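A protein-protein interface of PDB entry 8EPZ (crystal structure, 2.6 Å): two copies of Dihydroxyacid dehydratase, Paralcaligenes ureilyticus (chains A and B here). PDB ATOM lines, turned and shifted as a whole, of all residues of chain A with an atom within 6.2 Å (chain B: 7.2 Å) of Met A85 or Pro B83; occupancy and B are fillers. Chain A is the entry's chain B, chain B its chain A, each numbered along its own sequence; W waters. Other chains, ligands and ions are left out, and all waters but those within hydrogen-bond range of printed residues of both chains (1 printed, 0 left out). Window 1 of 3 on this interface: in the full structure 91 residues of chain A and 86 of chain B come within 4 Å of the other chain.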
ATOM      1  N   ASN A  49       1.342  19.754   3.764  1.00  0.00           N
ATOM      2  CA  ASN A  49       0.509  18.742   3.130  1.00  0.00           C
ATOM      3  C   ASN A  49       1.146  17.373   3.335  1.00  0.00           C
ATOM      4  O   ASN A  49       2.158  17.050   2.706  1.00  0.00           O
ATOM      5  CB  ASN A  49       0.326  19.032   1.644  1.00  0.00           C
ATOM      6  CG  ASN A  49      -0.903  18.358   1.070  1.00  0.00           C
ATOM      7  OD1 ASN A  49      -1.509  17.498   1.711  1.00  0.00           O
ATOM      8  ND2 ASN A  49      -1.282  18.750  -0.139  1.00  0.00           N
ATOM      9  N   THR A  50       0.545  16.571   4.208  1.00  0.00           N
ATOM     10  CA  THR A  50       0.939  15.184   4.391  1.00  0.00           C
ATOM     11  C   THR A  50       0.198  14.245   3.449  1.00  0.00           C
ATOM     12  O   THR A  50       0.071  13.052   3.750  1.00  0.00           O
ATOM     13  CB  THR A  50       0.714  14.764   5.843  1.00  0.00           C
ATOM     14  OG1 THR A  50      -0.683  14.845   6.150  1.00  0.00           O
ATOM     15  CG2 THR A  50       1.478  15.689   6.767  1.00  0.00           C
ATOM     16  N   PHE A  51      -0.305  14.761   2.328  1.00  0.00           N
ATOM     17  CA  PHE A  51      -0.946  13.911   1.335  1.00  0.00           C
ATOM     18  C   PHE A  51       0.038  12.874   0.815  1.00  0.00           C
ATOM     19  O   PHE A  51       1.204  13.178   0.553  1.00  0.00           O
ATOM     20  CB  PHE A  51      -1.477  14.751   0.172  1.00  0.00           C
ATOM     21  CG  PHE A  51      -1.633  13.980  -1.109  1.00  0.00           C
ATOM     22  CD1 PHE A  51      -2.723  13.147  -1.302  1.00  0.00           C
ATOM     23  CD2 PHE A  51      -0.688  14.084  -2.117  1.00  0.00           C
ATOM     24  CE1 PHE A  51      -2.869  12.430  -2.476  1.00  0.00           C
ATOM     25  CE2 PHE A  51      -0.827  13.369  -3.294  1.00  0.00           C
ATOM     26  CZ  PHE A  51      -1.921  12.543  -3.474  1.00  0.00           C
ATOM     27  N   SER A  52      -0.443  11.645   0.663  1.00  0.00           N
ATOM     28  CA  SER A  52       0.381  10.572   0.133  1.00  0.00           C
ATOM     29  C   SER A  52      -0.524   9.418  -0.267  1.00  0.00           C
ATOM     30  O   SER A  52      -1.516   9.142   0.409  1.00  0.00           O
ATOM     31  CB  SER A  52       1.416  10.098   1.159  1.00  0.00           C
ATOM     32  OG  SER A  52       2.340   9.200   0.568  1.00  0.00           O
ATOM     33  N   GLU A  53      -0.182   8.760  -1.373  1.00  0.00           N
ATOM     34  CA  GLU A  53      -0.858   7.524  -1.735  1.00  0.00           C
ATOM     35  C   GLU A  53      -0.329   6.332  -0.955  1.00  0.00           C
ATOM     36  O   GLU A  53      -0.933   5.255  -1.012  1.00  0.00           O
ATOM     37  CB  GLU A  53      -0.731   7.274  -3.236  1.00  0.00           C
ATOM     38  CG  GLU A  53      -1.720   8.081  -4.053  1.00  0.00           C
ATOM     39  CD  GLU A  53      -1.237   8.348  -5.455  1.00  0.00           C
ATOM     40  OE1 GLU A  53      -0.037   8.119  -5.722  1.00  0.00           O
ATOM     41  OE2 GLU A  53      -2.055   8.791  -6.289  1.00  0.00           O
ATOM     42  N   THR A  55      -0.053   6.913   2.288  1.00  0.00           N
ATOM     43  CA  THR A  55      -0.804   7.207   3.500  1.00  0.00           C
ATOM     44  C   THR A  55      -2.290   7.125   3.162  1.00  0.00           C
ATOM     45  O   THR A  55      -2.923   8.154   2.888  1.00  0.00           O
ATOM     46  CB  THR A  55      -0.437   8.586   4.050  1.00  0.00           C
ATOM     47  OG1 THR A  55       0.987   8.684   4.179  1.00  0.00           O
ATOM     48  CG2 THR A  55      -1.065   8.803   5.411  1.00  0.00           C
ATOM     49  N   PRO A  83       5.542  19.930   1.194  1.00  0.00           N
ATOM     50  CA  PRO A  83       5.419  18.554   1.679  1.00  0.00           C
ATOM     51  C   PRO A  83       6.398  18.229   2.790  1.00  0.00           C
ATOM     52  O   PRO A  83       7.409  18.915   2.979  1.00  0.00           O
ATOM     53  CB  PRO A  83       5.723  17.730   0.424  1.00  0.00           C
ATOM     54  CG  PRO A  83       6.678  18.620  -0.381  1.00  0.00           C
ATOM     55  CD  PRO A  83       6.624  20.029   0.204  1.00  0.00           C
ATOM     56  N   VAL A  84       6.088  17.176   3.537  1.00  0.00           N
ATOM     57  CA  VAL A  84       7.008  16.545   4.468  1.00  0.00           C
ATOM     58  C   VAL A  84       6.842  15.041   4.305  1.00  0.00           C
ATOM     59  O   VAL A  84       6.004  14.576   3.530  1.00  0.00           O
ATOM     60  CB  VAL A  84       6.765  16.981   5.930  1.00  0.00           C
ATOM     61  CG1 VAL A  84       6.979  18.484   6.087  1.00  0.00           C
ATOM     62  CG2 VAL A  84       5.363  16.594   6.376  1.00  0.00           C
ATOM     63  N   MET A  85       7.652  14.270   5.023  1.00  0.00           N
ATOM     64  CA  MET A  85       7.446  12.828   5.028  1.00  0.00           C
ATOM     65  C   MET A  85       6.088  12.513   5.636  1.00  0.00           C
ATOM     66  O   MET A  85       5.796  12.919   6.763  1.00  0.00           O
ATOM     67  CB  MET A  85       8.551  12.119   5.810  1.00  0.00           C
ATOM     68  CG  MET A  85       8.196  10.679   6.161  1.00  0.00           C
ATOM     69  SD  MET A  85       9.403   9.828   7.196  1.00  0.00           S
ATOM     70  CE  MET A  85      10.622   9.361   5.973  1.00  0.00           C
ATOM     71  N   SER A  86       5.245  11.822   4.878  1.00  0.00           N
ATOM     72  CA  SER A  86       3.966  11.364   5.394  1.00  0.00           C
ATOM     73  C   SER A  86       4.134   9.981   6.010  1.00  0.00           C
ATOM     74  O   SER A  86       4.977   9.187   5.581  1.00  0.00           O
ATOM     75  CB  SER A  86       2.910  11.333   4.289  1.00  0.00           C
ATOM     76  OG  SER A  86       1.618  11.092   4.822  1.00  0.00           O
ATOM     77  N   LEU A  87       3.379   9.692   7.049  1.00  0.00           N
ATOM     78  CA  LEU A  87       3.507   8.401   7.742  1.00  0.00           C
ATOM     79  C   LEU A  87       2.209   7.636   7.606  1.00  0.00           C
ATOM     80  O   LEU A  87       1.218   8.133   8.059  1.00  0.00           O
ATOM     81  CB  LEU A  87       3.743   8.657   9.229  1.00  0.00           C
ATOM     82  CG  LEU A  87       4.724   9.759   9.577  1.00  0.00           C
ATOM     83  CD1 LEU A  87       4.796   9.931  11.075  1.00  0.00           C
ATOM     84  CD2 LEU A  87       6.089   9.452   9.019  1.00  0.00           C
ATOM     85  N   LEU A  92       4.068   1.726   7.007  1.00  0.00           N
ATOM     86  CA  LEU A  92       5.483   1.876   7.419  1.00  0.00           C
ATOM     87  C   LEU A  92       5.917   0.702   8.287  1.00  0.00           C
ATOM     88  O   LEU A  92       5.142   0.278   9.108  1.00  0.00           O
ATOM     89  CB  LEU A  92       5.658   3.205   8.143  1.00  0.00           C
ATOM     90  CG  LEU A  92       5.985   4.384   7.243  1.00  0.00           C
ATOM     91  CD1 LEU A  92       6.030   5.652   8.048  1.00  0.00           C
ATOM     92  CD2 LEU A  92       7.302   4.189   6.554  1.00  0.00           C
ATOM     93  N   PHE A  99       9.609   6.708  12.492  1.00  0.00           N
ATOM     94  CA  PHE A  99       9.834   7.886  11.665  1.00  0.00           C
ATOM     95  C   PHE A  99       9.060   9.103  12.146  1.00  0.00           C
ATOM     96  O   PHE A  99       9.070  10.135  11.467  1.00  0.00           O
ATOM     97  CB  PHE A  99       9.477   7.566  10.213  1.00  0.00           C
ATOM     98  CG  PHE A  99       9.967   6.224   9.766  1.00  0.00           C
ATOM     99  CD1 PHE A  99       9.115   5.134   9.742  1.00  0.00           C
ATOM    100  CD2 PHE A  99      11.289   6.046   9.394  1.00  0.00           C
ATOM    101  CE1 PHE A  99       9.567   3.892   9.340  1.00  0.00           C
ATOM    102  CE2 PHE A  99      11.747   4.806   8.994  1.00  0.00           C
ATOM    103  CZ  PHE A  99      10.886   3.728   8.966  1.00  0.00           C
ATOM    104  N   LEU A 102      11.527  11.856  12.498  1.00  0.00           N
ATOM    105  CA  LEU A 102      12.126  12.300  11.243  1.00  0.00           C
ATOM    106  C   LEU A 102      11.211  13.270  10.505  1.00  0.00           C
ATOM    107  O   LEU A 102      11.679  14.275   9.958  1.00  0.00           O
ATOM    108  CB  LEU A 102      12.462  11.098  10.362  1.00  0.00           C
ATOM    109  CG  LEU A 102      13.044  11.424   8.985  1.00  0.00           C
ATOM    110  CD1 LEU A 102      14.286  12.299   9.105  1.00  0.00           C
ATOM    111  CD2 LEU A 102      13.365  10.144   8.238  1.00  0.00           C
ATOM    112  N   ALA A 103       9.904  12.991  10.485  1.00  0.00           N
ATOM    113  CA  ALA A 103       8.968  13.926   9.871  1.00  0.00           C
ATOM    114  C   ALA A 103       8.902  15.244  10.633  1.00  0.00           C
ATOM    115  O   ALA A 103       8.689  16.299  10.025  1.00  0.00           O
ATOM    116  CB  ALA A 103       7.579  13.301   9.779  1.00  0.00           C
ATOM    117  N   ASP A 106      11.376  17.569   9.273  1.00  0.00           N
ATOM    118  CA  ASP A 106      10.920  18.168   8.023  1.00  0.00           C
ATOM    119  C   ASP A 106      10.014  19.356   8.300  1.00  0.00           C
ATOM    120  O   ASP A 106      10.186  20.434   7.721  1.00  0.00           O
ATOM    121  CB  ASP A 106      10.187  17.142   7.161  1.00  0.00           C
ATOM    122  CG  ASP A 106      10.947  15.851   7.026  1.00  0.00           C
ATOM    123  OD1 ASP A 106      10.303  14.782   7.005  1.00  0.00           O
ATOM    124  OD2 ASP A 106      12.192  15.908   6.950  1.00  0.00           O
ATOM    125  N   THR A 128       0.901  11.042  11.825  1.00  0.00           N
ATOM    126  CA  THR A 128       1.073  12.341  11.126  1.00  0.00           C
ATOM    127  C   THR A 128       0.565  13.533  11.943  1.00  0.00           C
ATOM    128  O   THR A 128       0.889  14.641  11.602  1.00  0.00           O
ATOM    129  CB  THR A 128       0.444  12.241   9.748  1.00  0.00           C
ATOM    130  OG1 THR A 128       1.058  13.248   8.978  1.00  0.00           O
ATOM    131  CG2 THR A 128      -1.026  12.535   9.778  1.00  0.00           C
ATOM    132  N   SER A 131       3.610  14.429  14.305  1.00  0.00           N
ATOM    133  CA  SER A 131       4.767  14.810  13.498  1.00  0.00           C
ATOM    134  C   SER A 131       4.775  16.306  13.214  1.00  0.00           C
ATOM    135  O   SER A 131       5.814  16.970  13.338  1.00  0.00           O
ATOM    136  CB  SER A 131       4.772  14.023  12.187  1.00  0.00           C
ATOM    137  OG  SER A 131       4.225  12.733  12.361  1.00  0.00           O
ATOM    138  N   LEU A 132       3.617  16.854  12.849  1.00  0.00           N
ATOM    139  CA  LEU A 132       3.477  18.264  12.509  1.00  0.00           C
ATOM    140  C   LEU A 132       3.286  19.140  13.740  1.00  0.00           C
ATOM    141  O   LEU A 132       3.786  20.268  13.778  1.00  0.00           O
ATOM    142  CB  LEU A 132       2.302  18.454  11.550  1.00  0.00           C
ATOM    143  CG  LEU A 132       2.532  18.149  10.075  1.00  0.00           C
ATOM    144  CD1 LEU A 132       2.978  16.710   9.836  1.00  0.00           C
ATOM    145  CD2 LEU A 132       1.271  18.450   9.284  1.00  0.00           C
ATOM    146  N   ILE B  47       6.689   6.771  -6.345  1.00  0.00           N
ATOM    147  CA  ILE B  47       7.060   7.979  -7.075  1.00  0.00           C
ATOM    148  C   ILE B  47       7.319   9.069  -6.046  1.00  0.00           C
ATOM    149  O   ILE B  47       6.379   9.635  -5.476  1.00  0.00           O
ATOM    150  CB  ILE B  47       5.980   8.395  -8.080  1.00  0.00           C
ATOM    151  CG1 ILE B  47       5.617   7.214  -8.980  1.00  0.00           C
ATOM    152  CG2 ILE B  47       6.463   9.564  -8.926  1.00  0.00           C
ATOM    153  CD1 ILE B  47       4.366   7.433  -9.791  1.00  0.00           C
ATOM    154  N   CYS B  48       8.590   9.365  -5.796  1.00  0.00           N
ATOM    155  CA  CYS B  48       8.943  10.366  -4.796  1.00  0.00           C
ATOM    156  C   CYS B  48       8.728  11.749  -5.390  1.00  0.00           C
ATOM    157  O   CYS B  48       9.518  12.209  -6.221  1.00  0.00           O
ATOM    158  CB  CYS B  48      10.379  10.193  -4.324  1.00  0.00           C
ATOM    159  SG  CYS B  48      10.717  11.156  -2.837  1.00  0.00           S
ATOM    160  N   ASN B  49       7.666  12.417  -4.953  1.00  0.00           N
ATOM    161  CA  ASN B  49       7.253  13.697  -5.507  1.00  0.00           C
ATOM    162  C   ASN B  49       7.779  14.823  -4.627  1.00  0.00           C
ATOM    163  O   ASN B  49       7.412  14.923  -3.452  1.00  0.00           O
ATOM    164  CB  ASN B  49       5.730  13.764  -5.622  1.00  0.00           C
ATOM    165  CG  ASN B  49       5.255  15.008  -6.336  1.00  0.00           C
ATOM    166  OD1 ASN B  49       6.057  15.801  -6.825  1.00  0.00           O
ATOM    167  ND2 ASN B  49       3.940  15.180  -6.413  1.00  0.00           N
ATOM    168  N   THR B  50       8.633  15.671  -5.200  1.00  0.00           N
ATOM    169  CA  THR B  50       9.121  16.861  -4.522  1.00  0.00           C
ATOM    170  C   THR B  50       8.327  18.107  -4.896  1.00  0.00           C
ATOM    171  O   THR B  50       8.857  19.221  -4.817  1.00  0.00           O
ATOM    172  CB  THR B  50      10.608  17.072  -4.816  1.00  0.00           C
ATOM    173  OG1 THR B  50      10.839  17.003  -6.229  1.00  0.00           O
ATOM    174  CG2 THR B  50      11.446  16.016  -4.106  1.00  0.00           C
ATOM    175  N   PHE B  51       7.069  17.945  -5.303  1.00  0.00           N
ATOM    176  CA  PHE B  51       6.238  19.098  -5.615  1.00  0.00           C
ATOM    177  C   PHE B  51       6.004  19.944  -4.370  1.00  0.00           C
ATOM    178  O   PHE B  51       5.781  19.418  -3.277  1.00  0.00           O
ATOM    179  CB  PHE B  51       4.893  18.659  -6.193  1.00  0.00           C
ATOM    180  CG  PHE B  51       3.777  19.632  -5.921  1.00  0.00           C
ATOM    181  CD1 PHE B  51       3.630  20.771  -6.695  1.00  0.00           C
ATOM    182  CD2 PHE B  51       2.887  19.413  -4.880  1.00  0.00           C
ATOM    183  CE1 PHE B  51       2.611  21.672  -6.440  1.00  0.00           C
ATOM    184  CE2 PHE B  51       1.870  20.310  -4.619  1.00  0.00           C
ATOM    185  CZ  PHE B  51       1.730  21.439  -5.400  1.00  0.00           C
ATOM    186  N   GLU B  81       2.553   7.567  -5.307  1.00  0.00           N
ATOM    187  CA  GLU B  81       3.398   8.722  -5.052  1.00  0.00           C
ATOM    188  C   GLU B  81       3.433   9.012  -3.558  1.00  0.00           C
ATOM    189  O   GLU B  81       2.485   8.720  -2.823  1.00  0.00           O
ATOM    190  CB  GLU B  81       2.914   9.954  -5.824  1.00  0.00           C
ATOM    191  CG  GLU B  81       1.995  10.880  -5.045  1.00  0.00           C
ATOM    192  CD  GLU B  81       1.755  12.198  -5.758  1.00  0.00           C
ATOM    193  OE1 GLU B  81       0.967  12.225  -6.727  1.00  0.00           O
ATOM    194  OE2 GLU B  81       2.363  13.211  -5.351  1.00  0.00           O
ATOM    195  N   PHE B  82       4.552   9.571  -3.109  1.00  0.00           N
ATOM    196  CA  PHE B  82       4.715   9.897  -1.703  1.00  0.00           C
ATOM    197  C   PHE B  82       5.581  11.139  -1.588  1.00  0.00           C
ATOM    198  O   PHE B  82       6.423  11.388  -2.458  1.00  0.00           O
ATOM    199  CB  PHE B  82       5.331   8.728  -0.914  1.00  0.00           C
ATOM    200  CG  PHE B  82       6.737   8.388  -1.318  1.00  0.00           C
ATOM    201  CD1 PHE B  82       6.982   7.484  -2.338  1.00  0.00           C
ATOM    202  CD2 PHE B  82       7.818   8.960  -0.662  1.00  0.00           C
ATOM    203  CE1 PHE B  82       8.278   7.166  -2.705  1.00  0.00           C
ATOM    204  CE2 PHE B  82       9.112   8.649  -1.024  1.00  0.00           C
ATOM    205  CZ  PHE B  82       9.343   7.749  -2.045  1.00  0.00           C
ATOM    206  N   PRO B  83       5.388  11.943  -0.546  1.00  0.00           N
ATOM    207  CA  PRO B  83       6.155  13.179  -0.406  1.00  0.00           C
ATOM    208  C   PRO B  83       7.385  13.019   0.470  1.00  0.00           C
ATOM    209  O   PRO B  83       7.470  12.147   1.337  1.00  0.00           O
ATOM    210  CB  PRO B  83       5.145  14.119   0.263  1.00  0.00           C
ATOM    211  CG  PRO B  83       4.389  13.201   1.168  1.00  0.00           C
ATOM    212  CD  PRO B  83       4.297  11.872   0.441  1.00  0.00           C
ATOM    213  N   VAL B  84       8.355  13.890   0.210  1.00  0.00           N
ATOM    214  CA  VAL B  84       9.480  14.132   1.100  1.00  0.00           C
ATOM    215  C   VAL B  84       9.681  15.638   1.164  1.00  0.00           C
ATOM    216  O   VAL B  84       9.076  16.399   0.406  1.00  0.00           O
ATOM    217  CB  VAL B  84      10.776  13.437   0.636  1.00  0.00           C
ATOM    218  CG1 VAL B  84      10.590  11.927   0.615  1.00  0.00           C
ATOM    219  CG2 VAL B  84      11.194  13.969  -0.726  1.00  0.00           C
ATOM    220  N   MET B  85      10.538  16.071   2.083  1.00  0.00           N
ATOM    221  CA  MET B  85      10.823  17.493   2.189  1.00  0.00           C
ATOM    222  C   MET B  85      11.442  17.992   0.891  1.00  0.00           C
ATOM    223  O   MET B  85      12.417  17.421   0.393  1.00  0.00           O
ATOM    224  CB  MET B  85      11.752  17.773   3.366  1.00  0.00           C
ATOM    225  CG  MET B  85      11.852  19.252   3.696  1.00  0.00           C
ATOM    226  SD  MET B  85      12.688  19.595   5.254  1.00  0.00           S
ATOM    227  CE  MET B  85      14.360  19.844   4.683  1.00  0.00           C
ATOM    228  N   SER B  86      10.857  19.044   0.333  1.00  0.00           N
ATOM    229  CA  SER B  86      11.330  19.623  -0.914  1.00  0.00           C
ATOM    230  C   SER B  86      12.242  20.807  -0.626  1.00  0.00           C
ATOM    231  O   SER B  86      12.092  21.501   0.382  1.00  0.00           O
ATOM    232  CB  SER B  86      10.163  20.063  -1.797  1.00  0.00           C
ATOM    233  OG  SER B  86      10.611  20.292  -3.121  1.00  0.00           O
ATOM    234  N   MET B 105      17.363  11.633   4.267  1.00  0.00           N
ATOM    235  CA  MET B 105      16.806  10.634   5.172  1.00  0.00           C
ATOM    236  C   MET B 105      15.335  10.366   4.882  1.00  0.00           C
ATOM    237  O   MET B 105      14.869   9.235   5.062  1.00  0.00           O
ATOM    238  CB  MET B 105      16.992  11.075   6.623  1.00  0.00           C
ATOM    239  CG  MET B 105      18.432  11.020   7.091  1.00  0.00           C
ATOM    240  SD  MET B 105      18.629  11.145   8.879  1.00  0.00           S
ATOM    241  CE  MET B 105      18.272  12.878   9.141  1.00  0.00           C
ATOM    242  N   ASP B 106      14.589  11.382   4.435  1.00  0.00           N
ATOM    243  CA  ASP B 106      13.174  11.178   4.131  1.00  0.00           C
ATOM    244  C   ASP B 106      12.992  10.166   3.009  1.00  0.00           C
ATOM    245  O   ASP B 106      12.191   9.231   3.124  1.00  0.00           O
ATOM    246  CB  ASP B 106      12.504  12.499   3.752  1.00  0.00           C
ATOM    247  CG  ASP B 106      12.319  13.421   4.931  1.00  0.00           C
ATOM    248  OD1 ASP B 106      12.448  14.649   4.743  1.00  0.00           O
ATOM    249  OD2 ASP B 106      12.055  12.920   6.046  1.00  0.00           O
ATOM    250  N   VAL B 107      13.730  10.338   1.912  1.00  0.00           N
ATOM    251  CA  VAL B 107      13.539   9.472   0.755  1.00  0.00           C
ATOM    252  C   VAL B 107      13.991   8.051   1.068  1.00  0.00           C
ATOM    253  O   VAL B 107      13.355   7.078   0.649  1.00  0.00           O
ATOM    254  CB  VAL B 107      14.264  10.054  -0.475  1.00  0.00           C
ATOM    255  CG1 VAL B 107      13.799  11.469  -0.735  1.00  0.00           C
ATOM    256  CG2 VAL B 107      15.765  10.042  -0.288  1.00  0.00           C
ATOM    257  N   GLU B 108      15.071   7.907   1.837  1.00  0.00           N
ATOM    258  CA  GLU B 108      15.607   6.581   2.119  1.00  0.00           C
ATOM    259  C   GLU B 108      14.665   5.782   3.011  1.00  0.00           C
ATOM    260  O   GLU B 108      14.353   4.622   2.720  1.00  0.00           O
ATOM    261  CB  GLU B 108      16.980   6.704   2.769  1.00  0.00           C
ATOM    262  CG  GLU B 108      17.486   5.408   3.350  1.00  0.00           C
ATOM    263  CD  GLU B 108      18.851   5.561   3.958  1.00  0.00           C
ATOM    264  OE1 GLU B 108      19.361   6.701   3.992  1.00  0.00           O
ATOM    265  OE2 GLU B 108      19.421   4.544   4.404  1.00  0.00           O
ATOM    266  N   GLU B 109      14.210   6.384   4.109  1.00  0.00           N
ATOM    267  CA  GLU B 109      13.319   5.664   5.012  1.00  0.00           C
ATOM    268  C   GLU B 109      11.947   5.436   4.392  1.00  0.00           C
ATOM    269  O   GLU B 109      11.311   4.410   4.658  1.00  0.00           O
ATOM    270  CB  GLU B 109      13.190   6.421   6.331  1.00  0.00           C
ATOM    271  CG  GLU B 109      14.512   6.634   7.050  1.00  0.00           C
ATOM    272  CD  GLU B 109      15.320   5.358   7.179  1.00  0.00           C
ATOM    273  OE1 GLU B 109      16.527   5.386   6.856  1.00  0.00           O
ATOM    274  OE2 GLU B 109      14.748   4.328   7.592  1.00  0.00           O
ATOM    275  N   SER B 110      11.473   6.371   3.563  1.00  0.00           N
ATOM    276  CA  SER B 110      10.180   6.190   2.912  1.00  0.00           C
ATOM    277  C   SER B 110      10.191   5.047   1.909  1.00  0.00           C
ATOM    278  O   SER B 110       9.127   4.495   1.604  1.00  0.00           O
ATOM    279  CB  SER B 110       9.748   7.477   2.211  1.00  0.00           C
ATOM    280  OG  SER B 110       9.366   8.463   3.149  1.00  0.00           O
ATOM    281  N   ILE B 111      11.356   4.687   1.384  1.00  0.00           N
ATOM    282  CA  ILE B 111      11.444   3.581   0.436  1.00  0.00           C
ATOM    283  C   ILE B 111      11.582   2.244   1.159  1.00  0.00           C
ATOM    284  O   ILE B 111      11.003   1.240   0.735  1.00  0.00           O
ATOM    285  CB  ILE B 111      12.612   3.824  -0.543  1.00  0.00           C
ATOM    286  CG1 ILE B 111      12.324   5.040  -1.426  1.00  0.00           C
ATOM    287  CG2 ILE B 111      12.856   2.597  -1.402  1.00  0.00           C
ATOM    288  CD1 ILE B 111      13.529   5.519  -2.213  1.00  0.00           C
ATOM    289  N   ASN B 114       8.192   1.367   3.207  1.00  0.00           N
ATOM    290  CA  ASN B 114       6.978   1.207   2.423  1.00  0.00           C
ATOM    291  C   ASN B 114       7.127   0.075   1.411  1.00  0.00           C
ATOM    292  O   ASN B 114       8.232  -0.196   0.930  1.00  0.00           O
ATOM    293  CB  ASN B 114       6.621   2.503   1.685  1.00  0.00           C
ATOM    294  CG  ASN B 114       6.198   3.608   2.629  1.00  0.00           C
ATOM    295  OD1 ASN B 114       5.077   3.609   3.138  1.00  0.00           O
ATOM    296  ND2 ASN B 114       7.096   4.556   2.872  1.00  0.00           N
HETATM  297  O   HOH W   1       8.929  20.814   2.364  1.00  0.00           O
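Among the printed residues, merely in contact across the chains: Phe A51 with Glu B81, Phe A51 with Pro B83, Ser A52 with Phe B82, Ser A52 with Pro B83, Pro A83 with Phe B51, Pro A83 with Pro B83, Pro A83 with Val B84, Pro A83 with Met B85, Val A84 with Pro B83, Met A85 with Pro B83, Met A85 with Asp B106, Met A85 with Glu B109, Met A85 with Ser B110, Ser A86 with Pro B83, Leu A92 with Asn B114, Phe A99 with Glu B109, Leu A102 with Met B105, Leu A102 with Asp B106 and Leu A102 with Glu B109.
Water W1 bridges O of Pro A83 (2.5 Å) and N of Ser B86 (3.3 Å).
Phe A51 touches Pro B83, and with the chains exchanged Pro A83 touches Phe B51. Pro A83 touches Met B85, and with the chains exchanged Met A85 touches Pro B83. Ser A86 touches Pro B83, but with the chains exchanged Pro A83 does not touch Ser B86 (4.03 Å). Asp A106 touches its own counterpart, Asp B106. Positions printed for both chains: 49, 50, 51, 83, 84, 85, 86 and 106.
The side-chain amide oxygen (OD1) of Asn A49 sits at hydrogen-bond distance from the backbone NH (N) of Phe A51. The backbone carbonyl oxygen of Phe B82 sits at hydrogen-bond distance from the backbone NH of Asn B49 (3.0 Å). The backbone NH (N) of Met A85 is in hydrogen-bond range of the side-chain carboxylate (OD1) of Asp A106 (3.3 Å). The side-chain hydroxyl (OG) of Ser B110 sits at hydrogen-bond distance from the backbone carbonyl oxygen (O) of Asp B106. The backbone carbonyl oxygen of Thr A50 sits at hydrogen-bond distance from the side-chain hydroxyl of Ser A86 (2.7 Å). N of Phe B51 sits at hydrogen-bond distance from OD1 of Asn B49 (2.8 Å).
The backbone carbonyl oxygen (O) of Asp A106 sits close to the side-chain sulfur (SD) of Met B85 (3.6 Å). OG of Ser A52 lies within hydrogen-bond range of O of Glu B81, at 3.4 Å. N of Glu B81 lies within hydrogen-bond range of OE1 of Glu A53, 2.7 Å away. The side-chain carboxylate of Asp A106 sits close to the side-chain carboxylate of Asp B106, at 2.6 Å.
Printed residues of chain A that touch a printed residue of chain B: Phe A51, Ser A52, Glu A53, Pro A83, Val A84, Met A85, Ser A86, Leu A92, Phe A99, Leu A102 and Asp A106. Printed residues of chain B that touch a printed residue of chain A: Phe B51, Glu B81, Phe B82, Pro B83, Val B84, Met B85, Met B105, Asp B106, Glu B109, Ser B110 and Asn B114. Among the printed residues, 23 pairs touch across the chains.
Of the printed residues of chain B, Phe A51 touches Glu B81 and Pro B83. Met A85 touches four residues of chain B. Of the printed residues of chain B, Ser A86 touches Pro B83. Printed residues of chain B within 4 Å of Leu A102: Met B105, Asp B106 and Glu B109. Printed residues of chain A within 4 Å of Phe B51: Pro A83. Pro B83 touches six residues of chain A. The nearest printed residue of chain B that does not touch Met A85 is Val B84 (4.3 Å).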
